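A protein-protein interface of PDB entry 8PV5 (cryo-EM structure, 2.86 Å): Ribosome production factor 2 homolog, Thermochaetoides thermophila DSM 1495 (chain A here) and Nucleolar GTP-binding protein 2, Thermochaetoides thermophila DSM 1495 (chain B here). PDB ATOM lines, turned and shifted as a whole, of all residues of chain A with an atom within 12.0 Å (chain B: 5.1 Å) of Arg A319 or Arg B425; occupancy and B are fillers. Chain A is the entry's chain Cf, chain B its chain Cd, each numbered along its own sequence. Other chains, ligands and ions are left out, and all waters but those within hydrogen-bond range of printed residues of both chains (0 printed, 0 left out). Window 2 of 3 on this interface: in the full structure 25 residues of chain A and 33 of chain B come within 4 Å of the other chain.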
ATOM      1  N   THR A 311       8.376   6.793  -5.805  1.00  0.00           N
ATOM      2  CA  THR A 311       9.105   5.976  -6.757  1.00  0.00           C
ATOM      3  C   THR A 311      10.605   6.056  -6.487  1.00  0.00           C
ATOM      4  O   THR A 311      11.089   6.938  -5.773  1.00  0.00           O
ATOM      5  CB  THR A 311       8.807   6.422  -8.189  1.00  0.00           C
ATOM      6  OG1 THR A 311       8.965   7.841  -8.292  1.00  0.00           O
ATOM      7  CG2 THR A 311       7.383   6.053  -8.575  1.00  0.00           C
ATOM      8  N   ARG A 312      11.343   5.107  -7.056  1.00  0.00           N
ATOM      9  CA  ARG A 312      12.788   5.098  -6.886  1.00  0.00           C
ATOM     10  C   ARG A 312      13.419   6.236  -7.678  1.00  0.00           C
ATOM     11  O   ARG A 312      13.137   6.416  -8.866  1.00  0.00           O
ATOM     12  CB  ARG A 312      13.370   3.758  -7.326  1.00  0.00           C
ATOM     13  CG  ARG A 312      14.853   3.633  -7.049  1.00  0.00           C
ATOM     14  CD  ARG A 312      15.364   2.233  -7.296  1.00  0.00           C
ATOM     15  NE  ARG A 312      16.763   2.107  -6.908  1.00  0.00           N
ATOM     16  CZ  ARG A 312      17.178   1.823  -5.681  1.00  0.00           C
ATOM     17  NH1 ARG A 312      16.323   1.608  -4.695  1.00  0.00           N
ATOM     18  NH2 ARG A 312      18.483   1.754  -5.437  1.00  0.00           N
ATOM     19  N   LYS A 313      14.275   7.009  -7.008  1.00  0.00           N
ATOM     20  CA  LYS A 313      14.928   8.167  -7.618  1.00  0.00           C
ATOM     21  C   LYS A 313      16.214   7.710  -8.308  1.00  0.00           C
ATOM     22  O   LYS A 313      17.318   7.780  -7.766  1.00  0.00           O
ATOM     23  CB  LYS A 313      15.208   9.234  -6.567  1.00  0.00           C
ATOM     24  CG  LYS A 313      14.024   9.576  -5.677  1.00  0.00           C
ATOM     25  CD  LYS A 313      12.807   9.992  -6.483  1.00  0.00           C
ATOM     26  CE  LYS A 313      11.601  10.197  -5.583  1.00  0.00           C
ATOM     27  NZ  LYS A 313      10.345  10.333  -6.368  1.00  0.00           N
ATOM     28  N   MET A 314      16.051   7.231  -9.539  1.00  0.00           N
ATOM     29  CA  MET A 314      17.186   6.710 -10.287  1.00  0.00           C
ATOM     30  C   MET A 314      18.068   7.841 -10.804  1.00  0.00           C
ATOM     31  O   MET A 314      17.699   9.018 -10.772  1.00  0.00           O
ATOM     32  CB  MET A 314      16.718   5.853 -11.462  1.00  0.00           C
ATOM     33  CG  MET A 314      15.900   4.635 -11.086  1.00  0.00           C
ATOM     34  SD  MET A 314      14.854   4.104 -12.454  1.00  0.00           S
ATOM     35  CE  MET A 314      13.974   2.744 -11.707  1.00  0.00           C
ATOM     36  N   LYS A 315      19.255   7.461 -11.282  1.00  0.00           N
ATOM     37  CA  LYS A 315      20.189   8.435 -11.839  1.00  0.00           C
ATOM     38  C   LYS A 315      19.669   9.013 -13.148  1.00  0.00           C
ATOM     39  O   LYS A 315      19.889  10.192 -13.447  1.00  0.00           O
ATOM     40  CB  LYS A 315      21.555   7.782 -12.040  1.00  0.00           C
ATOM     41  CG  LYS A 315      22.675   8.744 -12.391  1.00  0.00           C
ATOM     42  CD  LYS A 315      23.983   7.999 -12.593  1.00  0.00           C
ATOM     43  CE  LYS A 315      25.160   8.954 -12.669  1.00  0.00           C
ATOM     44  NZ  LYS A 315      26.438   8.237 -12.932  1.00  0.00           N
ATOM     45  N   GLY A 316      18.972   8.198 -13.943  1.00  0.00           N
ATOM     46  CA  GLY A 316      18.476   8.657 -15.228  1.00  0.00           C
ATOM     47  C   GLY A 316      17.266   9.560 -15.144  1.00  0.00           C
ATOM     48  O   GLY A 316      16.891  10.170 -16.152  1.00  0.00           O
ATOM     49  N   LEU A 317      16.646   9.663 -13.971  1.00  0.00           N
ATOM     50  CA  LEU A 317      15.455  10.481 -13.787  1.00  0.00           C
ATOM     51  C   LEU A 317      15.779  11.907 -13.369  1.00  0.00           C
ATOM     52  O   LEU A 317      14.859  12.694 -13.135  1.00  0.00           O
ATOM     53  CB  LEU A 317      14.521   9.856 -12.744  1.00  0.00           C
ATOM     54  CG  LEU A 317      13.544   8.740 -13.135  1.00  0.00           C
ATOM     55  CD1 LEU A 317      12.552   9.231 -14.164  1.00  0.00           C
ATOM     56  CD2 LEU A 317      14.227   7.489 -13.615  1.00  0.00           C
ATOM     57  N   LYS A 318      17.057  12.256 -13.269  1.00  0.00           N
ATOM     58  CA  LYS A 318      17.483  13.566 -12.797  1.00  0.00           C
ATOM     59  C   LYS A 318      18.024  14.362 -13.976  1.00  0.00           C
ATOM     60  O   LYS A 318      18.893  13.878 -14.711  1.00  0.00           O
ATOM     61  CB  LYS A 318      18.543  13.421 -11.706  1.00  0.00           C
ATOM     62  CG  LYS A 318      18.121  12.507 -10.570  1.00  0.00           C
ATOM     63  CD  LYS A 318      19.265  12.235  -9.611  1.00  0.00           C
ATOM     64  CE  LYS A 318      18.832  11.297  -8.496  1.00  0.00           C
ATOM     65  NZ  LYS A 318      19.957  10.966  -7.579  1.00  0.00           N
ATOM     66  N   ARG A 319      17.516  15.577 -14.151  1.00  0.00           N
ATOM     67  CA  ARG A 319      17.924  16.425 -15.264  1.00  0.00           C
ATOM     68  C   ARG A 319      19.316  17.003 -15.032  1.00  0.00           C
ATOM     69  O   ARG A 319      19.696  17.293 -13.898  1.00  0.00           O
ATOM     70  CB  ARG A 319      16.912  17.556 -15.473  1.00  0.00           C
ATOM     71  CG  ARG A 319      17.249  18.545 -16.593  1.00  0.00           C
ATOM     72  CD  ARG A 319      17.108  17.940 -17.993  1.00  0.00           C
ATOM     73  NE  ARG A 319      18.301  17.232 -18.444  1.00  0.00           N
ATOM     74  CZ  ARG A 319      18.362  16.497 -19.547  1.00  0.00           C
ATOM     75  NH1 ARG A 319      17.309  16.341 -20.333  1.00  0.00           N
ATOM     76  NH2 ARG A 319      19.508  15.904 -19.869  1.00  0.00           N
ATOM     77  N   HIS B 421      17.205   9.505 -24.039  1.00  0.00           N
ATOM     78  CA  HIS B 421      17.582  10.513 -23.054  1.00  0.00           C
ATOM     79  C   HIS B 421      17.790   9.894 -21.678  1.00  0.00           C
ATOM     80  O   HIS B 421      18.626  10.367 -20.902  1.00  0.00           O
ATOM     81  CB  HIS B 421      16.525  11.616 -22.993  1.00  0.00           C
ATOM     82  CG  HIS B 421      15.139  11.110 -22.750  1.00  0.00           C
ATOM     83  ND1 HIS B 421      14.669  10.802 -21.491  1.00  0.00           N
ATOM     84  CD2 HIS B 421      14.118  10.861 -23.602  1.00  0.00           C
ATOM     85  CE1 HIS B 421      13.420  10.381 -21.580  1.00  0.00           C
ATOM     86  NE2 HIS B 421      13.061  10.409 -22.850  1.00  0.00           N
ATOM     87  N   HIS B 422      17.047   8.829 -21.365  1.00  0.00           N
ATOM     88  CA  HIS B 422      17.251   8.127 -20.101  1.00  0.00           C
ATOM     89  C   HIS B 422      18.636   7.493 -20.044  1.00  0.00           C
ATOM     90  O   HIS B 422      19.325   7.575 -19.022  1.00  0.00           O
ATOM     91  CB  HIS B 422      16.162   7.073 -19.903  1.00  0.00           C
ATOM     92  CG  HIS B 422      14.845   7.638 -19.468  1.00  0.00           C
ATOM     93  ND1 HIS B 422      14.745   8.727 -18.629  1.00  0.00           N
ATOM     94  CD2 HIS B 422      13.576   7.262 -19.748  1.00  0.00           C
ATOM     95  CE1 HIS B 422      13.470   9.000 -18.417  1.00  0.00           C
ATOM     96  NE2 HIS B 422      12.740   8.124 -19.083  1.00  0.00           N
ATOM     97  N   MET B 423      19.071   6.884 -21.150  1.00  0.00           N
ATOM     98  CA  MET B 423      20.417   6.319 -21.221  1.00  0.00           C
ATOM     99  C   MET B 423      21.479   7.411 -21.136  1.00  0.00           C
ATOM    100  O   MET B 423      22.526   7.230 -20.497  1.00  0.00           O
ATOM    101  CB  MET B 423      20.575   5.518 -22.514  1.00  0.00           C
ATOM    102  CG  MET B 423      20.212   4.050 -22.391  1.00  0.00           C
ATOM    103  SD  MET B 423      21.418   3.107 -21.443  1.00  0.00           S
ATOM    104  CE  MET B 423      20.947   1.436 -21.870  1.00  0.00           C
ATOM    105  N   GLU B 424      21.223   8.552 -21.785  1.00  0.00           N
ATOM    106  CA  GLU B 424      22.172   9.662 -21.756  1.00  0.00           C
ATOM    107  C   GLU B 424      22.342  10.219 -20.347  1.00  0.00           C
ATOM    108  O   GLU B 424      23.468  10.469 -19.907  1.00  0.00           O
ATOM    109  CB  GLU B 424      21.722  10.764 -22.716  1.00  0.00           C
ATOM    110  CG  GLU B 424      21.785  10.380 -24.184  1.00  0.00           C
ATOM    111  CD  GLU B 424      21.039  11.351 -25.076  1.00  0.00           C
ATOM    112  OE1 GLU B 424      20.255  12.164 -24.545  1.00  0.00           O
ATOM    113  OE2 GLU B 424      21.233  11.297 -26.307  1.00  0.00           O
ATOM    114  N   ARG B 425      21.240  10.401 -19.616  1.00  0.00           N
ATOM    115  CA  ARG B 425      21.350  10.892 -18.244  1.00  0.00           C
ATOM    116  C   ARG B 425      21.856   9.808 -17.301  1.00  0.00           C
ATOM    117  O   ARG B 425      22.397  10.113 -16.232  1.00  0.00           O
ATOM    118  CB  ARG B 425      20.008  11.444 -17.761  1.00  0.00           C
ATOM    119  CG  ARG B 425      19.406  12.501 -18.664  1.00  0.00           C
ATOM    120  CD  ARG B 425      18.349  13.313 -17.939  1.00  0.00           C
ATOM    121  NE  ARG B 425      17.205  12.498 -17.549  1.00  0.00           N
ATOM    122  CZ  ARG B 425      15.940  12.884 -17.656  1.00  0.00           C
ATOM    123  NH1 ARG B 425      15.619  14.070 -18.146  1.00  0.00           N
ATOM    124  NH2 ARG B 425      14.975  12.059 -17.261  1.00  0.00           N
ATOM    125  N   THR B 426      21.686   8.536 -17.671  1.00  0.00           N
ATOM    126  CA  THR B 426      22.197   7.457 -16.834  1.00  0.00           C
ATOM    127  C   THR B 426      23.715   7.367 -16.910  1.00  0.00           C
ATOM    128  O   THR B 426      24.389   7.263 -15.877  1.00  0.00           O
ATOM    129  CB  THR B 426      21.563   6.129 -17.251  1.00  0.00           C
ATOM    130  OG1 THR B 426      20.140   6.212 -17.106  1.00  0.00           O
ATOM    131  CG2 THR B 426      22.087   4.988 -16.392  1.00  0.00           C
ATOM    132  N   TYR B 427      24.278   7.418 -18.117  1.00  0.00           N
ATOM    133  CA  TYR B 427      25.700   7.152 -18.293  1.00  0.00           C
ATOM    134  C   TYR B 427      26.523   8.395 -18.617  1.00  0.00           C
ATOM    135  O   TYR B 427      27.735   8.270 -18.825  1.00  0.00           O
ATOM    136  CB  TYR B 427      25.910   6.093 -19.377  1.00  0.00           C
ATOM    137  CG  TYR B 427      25.529   4.700 -18.934  1.00  0.00           C
ATOM    138  CD1 TYR B 427      26.293   4.015 -18.000  1.00  0.00           C
ATOM    139  CD2 TYR B 427      24.414   4.064 -19.463  1.00  0.00           C
ATOM    140  CE1 TYR B 427      25.950   2.738 -17.597  1.00  0.00           C
ATOM    141  CE2 TYR B 427      24.066   2.788 -19.067  1.00  0.00           C
ATOM    142  CZ  TYR B 427      24.837   2.131 -18.134  1.00  0.00           C
ATOM    143  OH  TYR B 427      24.491   0.862 -17.737  1.00  0.00           O
ATOM    144  N   GLU B 428      25.902   9.580 -18.643  1.00  0.00           N
ATOM    145  CA  GLU B 428      26.559  10.852 -18.974  1.00  0.00           C
ATOM    146  C   GLU B 428      27.280  10.779 -20.320  1.00  0.00           C
ATOM    147  O   GLU B 428      28.414  11.236 -20.478  1.00  0.00           O
ATOM    148  CB  GLU B 428      27.511  11.292 -17.858  1.00  0.00           C
ATOM    149  CG  GLU B 428      26.839  12.076 -16.739  1.00  0.00           C
ATOM    150  CD  GLU B 428      26.281  11.186 -15.643  1.00  0.00           C
ATOM    151  OE1 GLU B 428      26.231   9.954 -15.833  1.00  0.00           O
ATOM    152  OE2 GLU B 428      25.889  11.724 -14.587  1.00  0.00           O
ATOM    153  N   ARG B 430      26.707  10.959 -24.763  1.00  0.00           N
ATOM    154  CA  ARG B 430      25.858  11.459 -25.836  1.00  0.00           C
ATOM    155  C   ARG B 430      26.643  11.430 -27.139  1.00  0.00           C
ATOM    156  O   ARG B 430      27.861  11.622 -27.155  1.00  0.00           O
ATOM    157  CB  ARG B 430      25.355  12.876 -25.521  1.00  0.00           C
ATOM    158  CG  ARG B 430      24.351  13.452 -26.511  1.00  0.00           C
ATOM    159  CD  ARG B 430      23.895  14.842 -26.102  1.00  0.00           C
ATOM    160  NE  ARG B 430      23.160  14.825 -24.844  1.00  0.00           N
ATOM    161  CZ  ARG B 430      23.592  15.368 -23.715  1.00  0.00           C
ATOM    162  NH1 ARG B 430      24.760  15.986 -23.650  1.00  0.00           N
ATOM    163  NH2 ARG B 430      22.835  15.289 -22.625  1.00  0.00           N
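The guanidinium group (NE) of Arg B425 lies within hydrogen-bond range of the backbone carbonyl oxygen (O) of Gly A316 (2.7 Å).
NZ of Lys A315 lies within salt-bridge range of OE1 of Glu B428, at 3.4 Å.
O of His B422 sits at hydrogen-bond distance from OG1 of Thr B426 (2.5 Å).
Lys A315 touches Arg B425 (O to O, 3.7 Å).
O of Thr B426 touches CD of Lys A315, at 3.4 Å.
O of Gly A316 touches ND1 of His B422, at 3.6 Å.
Gly A316 touches Thr B426 (CA to OG1, 3.5 Å).
CA of Leu A317 touches NH2 of Arg B425, at 3.8 Å.
Arg B425 touches Lys A318.
CD of Arg B425 touches NH2 of Arg A319, 3.4 Å away.
Thr A311 touches none of the printed residues of chain B.
Arg A312 touches none of the printed residues of chain B.
Printed residues of chain B within 4 Å of Leu A317: Arg B425.
Of the printed residues of chain B, Lys A318 touches Arg B425 (3.3 Å).
Arg A319 touches one residue of chain B.
No residue of chain A comes within 4 Å of His B421.
No residue of chain A comes within 4 Å of Glu B424.
Of chain A, only Lys A315, Gly A316, Leu A317, Lys A318 and Arg A319 come within 4 Å of Arg B425.
The nearest residue of chain B that does not touch Arg A319 is Arg B430 (4.4 Å).
The nearest printed residue of chain B that does not touch Gly A316 is His B421 (5.1 Å).
Hydrophobic or aromatic side chains of chain B that line the printed part of chain A: His B422.
Of the 9 printed residues of chain A, 5 touch a printed residue of chain B.
Among the printed residues, Asp or Glu carboxylates within 4 Å of a Lys or Arg side-chain nitrogen of the other chain: Lys A315 with Glu B428 (3.4 Å).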
